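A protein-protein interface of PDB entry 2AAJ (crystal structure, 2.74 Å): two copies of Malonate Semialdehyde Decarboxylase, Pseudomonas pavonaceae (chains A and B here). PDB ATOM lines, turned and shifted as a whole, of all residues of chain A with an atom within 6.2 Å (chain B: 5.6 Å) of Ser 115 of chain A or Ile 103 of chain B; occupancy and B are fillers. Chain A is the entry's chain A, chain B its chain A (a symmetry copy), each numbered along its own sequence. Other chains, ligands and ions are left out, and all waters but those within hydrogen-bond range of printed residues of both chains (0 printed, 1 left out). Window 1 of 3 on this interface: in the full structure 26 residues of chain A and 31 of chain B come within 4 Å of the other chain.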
ATOM      1  N   TYR A  39     -39.329   1.327   0.113  1.00  0.00           N
ATOM      2  CA  TYR A  39     -38.266   2.004  -0.632  1.00  0.00           C
ATOM      3  C   TYR A  39     -38.511   1.833  -2.111  1.00  0.00           C
ATOM      4  O   TYR A  39     -38.335   0.724  -2.642  1.00  0.00           O
ATOM      5  CB  TYR A  39     -36.899   1.444  -0.227  1.00  0.00           C
ATOM      6  CG  TYR A  39     -36.629   1.605   1.249  1.00  0.00           C
ATOM      7  CD1 TYR A  39     -36.032   2.766   1.727  1.00  0.00           C
ATOM      8  CD2 TYR A  39     -37.024   0.625   2.166  1.00  0.00           C
ATOM      9  CE1 TYR A  39     -35.836   2.953   3.104  1.00  0.00           C
ATOM     10  CE2 TYR A  39     -36.829   0.788   3.516  1.00  0.00           C
ATOM     11  CZ  TYR A  39     -36.236   1.947   3.997  1.00  0.00           C
ATOM     12  OH  TYR A  39     -36.015   2.104   5.343  1.00  0.00           O
ATOM     13  N   ALA A 112     -25.306  -7.572   5.034  1.00  0.00           N
ATOM     14  CA  ALA A 112     -24.219  -6.613   5.103  1.00  0.00           C
ATOM     15  C   ALA A 112     -24.405  -5.509   4.067  1.00  0.00           C
ATOM     16  O   ALA A 112     -23.752  -4.478   4.137  1.00  0.00           O
ATOM     17  CB  ALA A 112     -22.858  -7.343   4.908  1.00  0.00           C
ATOM     18  N   ASP A 113     -25.333  -5.718   3.139  1.00  0.00           N
ATOM     19  CA  ASP A 113     -25.431  -4.897   1.956  1.00  0.00           C
ATOM     20  C   ASP A 113     -26.454  -3.776   2.049  1.00  0.00           C
ATOM     21  O   ASP A 113     -26.817  -3.210   1.018  1.00  0.00           O
ATOM     22  CB  ASP A 113     -25.709  -5.791   0.736  1.00  0.00           C
ATOM     23  CG  ASP A 113     -24.591  -6.812   0.467  1.00  0.00           C
ATOM     24  OD1 ASP A 113     -23.412  -6.518   0.777  1.00  0.00           O
ATOM     25  OD2 ASP A 113     -24.799  -7.937  -0.057  1.00  0.00           O
ATOM     26  N   TRP A 114     -26.906  -3.470   3.263  1.00  0.00           N
ATOM     27  CA  TRP A 114     -27.939  -2.458   3.500  1.00  0.00           C
ATOM     28  C   TRP A 114     -27.553  -1.523   4.636  1.00  0.00           C
ATOM     29  O   TRP A 114     -27.010  -1.954   5.679  1.00  0.00           O
ATOM     30  CB  TRP A 114     -29.260  -3.096   3.856  1.00  0.00           C
ATOM     31  CG  TRP A 114     -29.825  -3.924   2.753  1.00  0.00           C
ATOM     32  CD1 TRP A 114     -29.613  -5.268   2.527  1.00  0.00           C
ATOM     33  CD2 TRP A 114     -30.712  -3.487   1.708  1.00  0.00           C
ATOM     34  NE1 TRP A 114     -30.312  -5.680   1.415  1.00  0.00           N
ATOM     35  CE2 TRP A 114     -31.005  -4.612   0.900  1.00  0.00           C
ATOM     36  CE3 TRP A 114     -31.305  -2.253   1.378  1.00  0.00           C
ATOM     37  CZ2 TRP A 114     -31.840  -4.531  -0.229  1.00  0.00           C
ATOM     38  CZ3 TRP A 114     -32.155  -2.185   0.288  1.00  0.00           C
ATOM     39  CH2 TRP A 114     -32.399  -3.308  -0.517  1.00  0.00           C
ATOM     40  N   SER A 115     -27.819  -0.238   4.444  1.00  0.00           N
ATOM     41  CA  SER A 115     -27.717   0.746   5.506  1.00  0.00           C
ATOM     42  C   SER A 115     -28.841   1.737   5.257  1.00  0.00           C
ATOM     43  O   SER A 115     -28.859   2.447   4.238  1.00  0.00           O
ATOM     44  CB  SER A 115     -26.358   1.454   5.454  1.00  0.00           C
ATOM     45  OG  SER A 115     -26.381   2.684   6.181  1.00  0.00           O
ATOM     46  N   PHE A 116     -29.781   1.762   6.179  1.00  0.00           N
ATOM     47  CA  PHE A 116     -30.995   2.542   6.021  1.00  0.00           C
ATOM     48  C   PHE A 116     -30.924   3.959   6.525  1.00  0.00           C
ATOM     49  O   PHE A 116     -31.809   4.752   6.218  1.00  0.00           O
ATOM     50  CB  PHE A 116     -32.205   1.803   6.606  1.00  0.00           C
ATOM     51  CG  PHE A 116     -32.490   0.539   5.889  1.00  0.00           C
ATOM     52  CD1 PHE A 116     -33.063   0.561   4.608  1.00  0.00           C
ATOM     53  CD2 PHE A 116     -32.126  -0.678   6.429  1.00  0.00           C
ATOM     54  CE1 PHE A 116     -33.300  -0.627   3.896  1.00  0.00           C
ATOM     55  CE2 PHE A 116     -32.365  -1.864   5.740  1.00  0.00           C
ATOM     56  CZ  PHE A 116     -32.950  -1.847   4.473  1.00  0.00           C
ATOM     57  N   GLY A 117     -29.886   4.271   7.281  1.00  0.00           N
ATOM     58  CA  GLY A 117     -29.689   5.592   7.844  1.00  0.00           C
ATOM     59  C   GLY A 117     -28.462   5.595   8.733  1.00  0.00           C
ATOM     60  O   GLY A 117     -28.017   4.552   9.258  1.00  0.00           O
ATOM     61  N   ARG A 118     -27.875   6.775   8.833  1.00  0.00           N
ATOM     62  CA  ARG A 118     -26.800   7.042   9.773  1.00  0.00           C
ATOM     63  C   ARG A 118     -25.527   6.245   9.572  1.00  0.00           C
ATOM     64  O   ARG A 118     -24.763   6.120  10.517  1.00  0.00           O
ATOM     65  CB  ARG A 118     -27.285   6.787  11.197  1.00  0.00           C
ATOM     66  CG  ARG A 118     -28.415   7.607  11.613  1.00  0.00           C
ATOM     67  CD  ARG A 118     -28.185   8.089  13.003  1.00  0.00           C
ATOM     68  NE  ARG A 118     -29.484   8.189  13.640  1.00  0.00           N
ATOM     69  CZ  ARG A 118     -30.167   9.315  13.676  1.00  0.00           C
ATOM     70  NH1 ARG A 118     -29.584  10.417  13.132  1.00  0.00           N
ATOM     71  NH2 ARG A 118     -31.394   9.324  14.237  1.00  0.00           N
ATOM     72  N   GLY A 119     -25.302   5.700   8.377  1.00  0.00           N
ATOM     73  CA  GLY A 119     -24.095   4.948   8.087  1.00  0.00           C
ATOM     74  C   GLY A 119     -24.052   3.683   8.931  1.00  0.00           C
ATOM     75  O   GLY A 119     -22.946   3.114   9.137  1.00  0.00           O
ATOM     76  N   ARG A 120     -25.237   3.257   9.424  1.00  0.00           N
ATOM     77  CA  ARG A 120     -25.400   2.051  10.253  1.00  0.00           C
ATOM     78  C   ARG A 120     -25.761   0.895   9.346  1.00  0.00           C
ATOM     79  O   ARG A 120     -26.561   1.086   8.423  1.00  0.00           O
ATOM     80  CB  ARG A 120     -26.535   2.248  11.264  1.00  0.00           C
ATOM     81  CG  ARG A 120     -26.196   3.163  12.421  1.00  0.00           C
ATOM     82  CD  ARG A 120     -27.350   3.436  13.345  1.00  0.00           C
ATOM     83  NE  ARG A 120     -27.045   4.476  14.334  1.00  0.00           N
ATOM     84  CZ  ARG A 120     -27.959   5.078  15.124  1.00  0.00           C
ATOM     85  NH1 ARG A 120     -29.245   4.750  15.017  1.00  0.00           N
ATOM     86  NH2 ARG A 120     -27.588   6.032  15.997  1.00  0.00           N
ATOM     87  N   ALA A 121     -25.190  -0.291   9.589  1.00  0.00           N
ATOM     88  CA  ALA A 121     -25.616  -1.546   8.936  1.00  0.00           C
ATOM     89  C   ALA A 121     -26.634  -2.305   9.824  1.00  0.00           C
ATOM     90  O   ALA A 121     -26.251  -3.201  10.588  1.00  0.00           O
ATOM     91  CB  ALA A 121     -24.403  -2.412   8.642  1.00  0.00           C
ATOM     92  N   GLU A 122     -27.917  -1.954   9.742  1.00  0.00           N
ATOM     93  CA  GLU A 122     -28.904  -2.395  10.747  1.00  0.00           C
ATOM     94  C   GLU A 122     -29.154  -3.894  10.850  1.00  0.00           C
ATOM     95  O   GLU A 122     -29.606  -4.378  11.897  1.00  0.00           O
ATOM     96  CB  GLU A 122     -30.236  -1.669  10.590  1.00  0.00           C
ATOM     97  CG  GLU A 122     -30.078  -0.170  10.722  1.00  0.00           C
ATOM     98  CD  GLU A 122     -29.903   0.552   9.402  1.00  0.00           C
ATOM     99  OE1 GLU A 122     -29.541  -0.096   8.395  1.00  0.00           O
ATOM    100  OE2 GLU A 122     -30.144   1.770   9.382  1.00  0.00           O
ATOM    101  N   LEU B  52     -39.516   6.866   0.188  1.00  0.00           N
ATOM    102  CA  LEU B  52     -38.468   6.278   1.003  1.00  0.00           C
ATOM    103  C   LEU B  52     -38.813   6.464   2.472  1.00  0.00           C
ATOM    104  O   LEU B  52     -38.702   7.572   3.015  1.00  0.00           O
ATOM    105  CB  LEU B  52     -37.114   6.926   0.685  1.00  0.00           C
ATOM    106  CG  LEU B  52     -36.647   6.922  -0.751  1.00  0.00           C
ATOM    107  CD1 LEU B  52     -35.582   7.982  -0.911  1.00  0.00           C
ATOM    108  CD2 LEU B  52     -36.156   5.527  -1.108  1.00  0.00           C
ATOM    109  N   GLU B  53     -39.219   5.378   3.108  1.00  0.00           N
ATOM    110  CA  GLU B  53     -39.541   5.417   4.542  1.00  0.00           C
ATOM    111  C   GLU B  53     -38.365   4.978   5.442  1.00  0.00           C
ATOM    112  O   GLU B  53     -37.227   5.196   5.076  1.00  0.00           O
ATOM    113  CB  GLU B  53     -40.849   4.694   4.839  1.00  0.00           C
ATOM    114  CG  GLU B  53     -42.022   5.399   4.198  1.00  0.00           C
ATOM    115  CD  GLU B  53     -43.321   4.702   4.495  1.00  0.00           C
ATOM    116  OE1 GLU B  53     -43.389   3.945   5.512  1.00  0.00           O
ATOM    117  OE2 GLU B  53     -44.272   4.926   3.722  1.00  0.00           O
ATOM    118  N   ARG B  61     -36.207  11.882   7.599  1.00  0.00           N
ATOM    119  CA  ARG B  61     -35.981  12.142   6.142  1.00  0.00           C
ATOM    120  C   ARG B  61     -36.526  13.463   5.633  1.00  0.00           C
ATOM    121  O   ARG B  61     -37.649  13.842   5.964  1.00  0.00           O
ATOM    122  CB  ARG B  61     -36.439  11.025   5.187  1.00  0.00           C
ATOM    123  CG  ARG B  61     -36.681   9.696   5.812  1.00  0.00           C
ATOM    124  CD  ARG B  61     -36.091   8.495   5.065  1.00  0.00           C
ATOM    125  NE  ARG B  61     -34.708   8.287   5.455  1.00  0.00           N
ATOM    126  CZ  ARG B  61     -34.118   7.098   5.721  1.00  0.00           C
ATOM    127  NH1 ARG B  61     -34.749   5.912   5.685  1.00  0.00           N
ATOM    128  NH2 ARG B  61     -32.827   7.124   6.033  1.00  0.00           N
ATOM    129  N   VAL B  65     -32.987  13.710   0.934  1.00  0.00           N
ATOM    130  CA  VAL B  65     -32.696  12.292   0.974  1.00  0.00           C
ATOM    131  C   VAL B  65     -31.926  11.813  -0.279  1.00  0.00           C
ATOM    132  O   VAL B  65     -32.275  12.157  -1.399  1.00  0.00           O
ATOM    133  CB  VAL B  65     -33.961  11.430   1.277  1.00  0.00           C
ATOM    134  CG1 VAL B  65     -34.984  11.451   0.120  1.00  0.00           C
ATOM    135  CG2 VAL B  65     -33.521   9.994   1.712  1.00  0.00           C
ATOM    136  N   VAL B  66     -30.873  11.039  -0.049  1.00  0.00           N
ATOM    137  CA  VAL B  66     -30.044  10.477  -1.085  1.00  0.00           C
ATOM    138  C   VAL B  66     -30.118   8.970  -0.989  1.00  0.00           C
ATOM    139  O   VAL B  66     -29.733   8.391   0.040  1.00  0.00           O
ATOM    140  CB  VAL B  66     -28.551  10.903  -0.858  1.00  0.00           C
ATOM    141  CG1 VAL B  66     -27.578  10.172  -1.822  1.00  0.00           C
ATOM    142  CG2 VAL B  66     -28.394  12.454  -0.927  1.00  0.00           C
ATOM    143  N   LEU B  67     -30.611   8.328  -2.047  1.00  0.00           N
ATOM    144  CA  LEU B  67     -30.580   6.858  -2.133  1.00  0.00           C
ATOM    145  C   LEU B  67     -29.420   6.424  -3.045  1.00  0.00           C
ATOM    146  O   LEU B  67     -29.325   6.858  -4.216  1.00  0.00           O
ATOM    147  CB  LEU B  67     -31.907   6.301  -2.656  1.00  0.00           C
ATOM    148  CG  LEU B  67     -31.902   4.831  -3.158  1.00  0.00           C
ATOM    149  CD1 LEU B  67     -31.739   3.840  -2.057  1.00  0.00           C
ATOM    150  CD2 LEU B  67     -33.113   4.427  -4.020  1.00  0.00           C
ATOM    151  N   LEU B  68     -28.567   5.547  -2.534  1.00  0.00           N
ATOM    152  CA  LEU B  68     -27.396   5.133  -3.269  1.00  0.00           C
ATOM    153  C   LEU B  68     -27.418   3.633  -3.550  1.00  0.00           C
ATOM    154  O   LEU B  68     -27.540   2.835  -2.608  1.00  0.00           O
ATOM    155  CB  LEU B  68     -26.161   5.511  -2.462  1.00  0.00           C
ATOM    156  CG  LEU B  68     -24.851   5.007  -3.044  1.00  0.00           C
ATOM    157  CD1 LEU B  68     -24.634   5.524  -4.448  1.00  0.00           C
ATOM    158  CD2 LEU B  68     -23.662   5.434  -2.123  1.00  0.00           C
ATOM    159  N   THR B  69     -27.275   3.244  -4.823  1.00  0.00           N
ATOM    160  CA  THR B  69     -27.153   1.811  -5.177  1.00  0.00           C
ATOM    161  C   THR B  69     -25.725   1.545  -5.609  1.00  0.00           C
ATOM    162  O   THR B  69     -25.165   2.272  -6.434  1.00  0.00           O
ATOM    163  CB  THR B  69     -28.122   1.402  -6.317  1.00  0.00           C
ATOM    164  OG1 THR B  69     -29.466   1.747  -5.963  1.00  0.00           O
ATOM    165  CG2 THR B  69     -28.168  -0.133  -6.500  1.00  0.00           C
ATOM    166  N   TYR B  84     -20.167   2.804   4.892  1.00  0.00           N
ATOM    167  CA  TYR B  84     -21.359   3.527   5.280  1.00  0.00           C
ATOM    168  C   TYR B  84     -21.056   4.655   6.234  1.00  0.00           C
ATOM    169  O   TYR B  84     -21.637   5.735   6.054  1.00  0.00           O
ATOM    170  CB  TYR B  84     -22.418   2.620   5.906  1.00  0.00           C
ATOM    171  CG  TYR B  84     -22.738   1.386   5.114  1.00  0.00           C
ATOM    172  CD1 TYR B  84     -22.905   1.451   3.728  1.00  0.00           C
ATOM    173  CD2 TYR B  84     -22.848   0.134   5.737  1.00  0.00           C
ATOM    174  CE1 TYR B  84     -23.185   0.326   2.979  1.00  0.00           C
ATOM    175  CE2 TYR B  84     -23.119  -1.045   4.969  1.00  0.00           C
ATOM    176  CZ  TYR B  84     -23.293  -0.929   3.589  1.00  0.00           C
ATOM    177  OH  TYR B  84     -23.566  -2.044   2.788  1.00  0.00           O
ATOM    178  N   ASP B 101     -30.566  11.230   6.152  1.00  0.00           N
ATOM    179  CA  ASP B 101     -31.037  11.382   4.796  1.00  0.00           C
ATOM    180  C   ASP B 101     -30.216  10.546   3.782  1.00  0.00           C
ATOM    181  O   ASP B 101     -30.221  10.864   2.581  1.00  0.00           O
ATOM    182  CB  ASP B 101     -30.931  12.850   4.429  1.00  0.00           C
ATOM    183  CG  ASP B 101     -32.225  13.591   4.569  1.00  0.00           C
ATOM    184  OD1 ASP B 101     -33.284  12.923   4.476  1.00  0.00           O
ATOM    185  OD2 ASP B 101     -32.275  14.853   4.739  1.00  0.00           O
ATOM    186  N   VAL B 102     -29.508   9.503   4.254  1.00  0.00           N
ATOM    187  CA  VAL B 102     -28.619   8.696   3.405  1.00  0.00           C
ATOM    188  C   VAL B 102     -28.994   7.212   3.524  1.00  0.00           C
ATOM    189  O   VAL B 102     -28.891   6.629   4.630  1.00  0.00           O
ATOM    190  CB  VAL B 102     -27.081   8.843   3.762  1.00  0.00           C
ATOM    191  CG1 VAL B 102     -26.213   7.963   2.851  1.00  0.00           C
ATOM    192  CG2 VAL B 102     -26.597  10.298   3.769  1.00  0.00           C
ATOM    193  N   ILE B 103     -29.411   6.620   2.384  1.00  0.00           N
ATOM    194  CA  ILE B 103     -29.789   5.205   2.267  1.00  0.00           C
ATOM    195  C   ILE B 103     -28.906   4.522   1.211  1.00  0.00           C
ATOM    196  O   ILE B 103     -28.739   5.055   0.107  1.00  0.00           O
ATOM    197  CB  ILE B 103     -31.265   5.103   1.849  1.00  0.00           C
ATOM    198  CG1 ILE B 103     -32.139   5.842   2.847  1.00  0.00           C
ATOM    199  CG2 ILE B 103     -31.712   3.666   1.663  1.00  0.00           C
ATOM    200  CD1 ILE B 103     -33.423   6.281   2.218  1.00  0.00           C
ATOM    201  N   VAL B 104     -28.354   3.353   1.563  1.00  0.00           N
ATOM    202  CA  VAL B 104     -27.440   2.606   0.695  1.00  0.00           C
ATOM    203  C   VAL B 104     -27.875   1.125   0.578  1.00  0.00           C
ATOM    204  O   VAL B 104     -28.138   0.441   1.592  1.00  0.00           O
ATOM    205  CB  VAL B 104     -25.980   2.575   1.248  1.00  0.00           C
ATOM    206  CG1 VAL B 104     -25.020   2.039   0.209  1.00  0.00           C
ATOM    207  CG2 VAL B 104     -25.544   3.880   1.791  1.00  0.00           C
ATOM    208  N   ALA B 105     -27.911   0.635  -0.655  1.00  0.00           N
ATOM    209  CA  ALA B 105     -28.197  -0.763  -0.937  1.00  0.00           C
ATOM    210  C   ALA B 105     -27.055  -1.232  -1.819  1.00  0.00           C
ATOM    211  O   ALA B 105     -26.672  -0.510  -2.715  1.00  0.00           O
ATOM    212  CB  ALA B 105     -29.522  -0.908  -1.661  1.00  0.00           C
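OH of Tyr 39 of chain A lies close to O of Glu 53 of chain B, at 3.3 Å. The backbone carbonyl oxygen (O) of Ser 115 of chain A lies within hydrogen-bond range of the backbone NH (N) of Val 104 of chain B (2.9 Å). The backbone carbonyl oxygen of Phe 116 of chain A sits at hydrogen-bond distance from the guanidinium group of Arg 61 of chain B. The backbone carbonyl oxygen of Ala 112 of chain A is in hydrogen-bond range of the side-chain hydroxyl of Tyr 84 of chain B (2.8 Å).
N of Phe 116 of chain A is in hydrogen-bond range of OE1 of Glu 122 of chain A (2.9 Å). The backbone carbonyl oxygen of Ile 103 of chain B lies within hydrogen-bond range of the backbone NH of Leu 68 of chain B, at 2.7 Å. The backbone NH (N) of Gly 117 of chain A sits at hydrogen-bond distance from the side-chain carboxylate (OE2) of Glu 122 of chain A (3.3 Å). The backbone NH of Ile 103 of chain B is in hydrogen-bond range of the backbone carbonyl oxygen of Val 66 of chain B (3.0 Å). The backbone carbonyl oxygen (O) of Glu 53 of chain B sits at hydrogen-bond distance from the guanidinium group (NH1) of Arg 61 of chain B, 2.7 Å away. The backbone carbonyl oxygen (O) of Leu 68 of chain B is in hydrogen-bond range of the backbone NH (N) of Ala 105 of chain B (3.0 Å).
Asp 113 of chain A touches Val 104 of chain B. O of Asp 113 of chain A touches CA of Ala 105 of chain B (3.4 Å). OH of Tyr 84 of chain B touches N of Trp 114 of chain A, 3.7 Å away. Val 104 of chain B touches Trp 114 of chain A (O to CA, 3.5 Å). Ala 105 of chain B touches Trp 114 of chain A (CB to CZ3, 3.5 Å). CG of Tyr 84 of chain B touches CB of Ser 115 of chain A (3.6 Å). CA of Ile 103 of chain B touches O of Ser 115 of chain A (3.5 Å). O of Val 102 of chain B touches O of Phe 116 of chain A (3.8 Å). Val 102 of chain B touches Gly 117 of chain A (O to CA, 3.5 Å). Tyr 84 of chain B touches Gly 119 of chain A (O to CA, 3.3 Å).
Of chain B, only Tyr 84 (3.6 Å), Ile 103 (3.5 Å) and Val 104 (2.9 Å) come within 4 Å of Ser 115 of chain A. Ile 103 of chain B touches two residues of chain A. Of the printed residues of chain B, Gly 117 of chain A touches Arg 61 (3.9 Å) and Val 102 (3.5 Å). Of the printed residues of chain A, Arg 61 of chain B touches Phe 116 (2.6 Å) and Gly 117 (3.9 Å). Printed residues of chain B within 4 Å of Tyr 39 of chain A: Leu 52 (3.96 Å) and Glu 53 (3.3 Å). Of the printed residues of chain B, Trp 114 of chain A touches Tyr 84, Val 104 and Ala 105. Printed residues of chain B within 4 Å of Ala 112 of chain A: Tyr 84 (2.8 Å). Val 66 of chain B touches none of the printed residues of chain A. Thr 69 of chain B touches none of the printed residues of chain A. The nearest residue of chain A that does not touch Ile 103 of chain B is Tyr 39 of chain A (4.2 Å).
Along chain A the printed residues that touch a printed residue of chain B span positions 39 to 119. Of the 14 printed residues of chain B, 8 touch a printed residue of chain A. Printed residues of chain B that touch a printed residue of chain A: Leu 52, Glu 53, Arg 61, Tyr 84, Val 102, Ile 103, Val 104 and Ala 105. Among the printed residues, 18 pairs touch across the chains. Among the printed residues, no Asp or Glu carboxylate lies within 4 Å of a Lys or Arg side-chain nitrogen of the other chain.
No position is printed for both chains. Of the 18 pairs that touch across the chains among the printed residues, none has its exchanged pair printed and touching as well.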
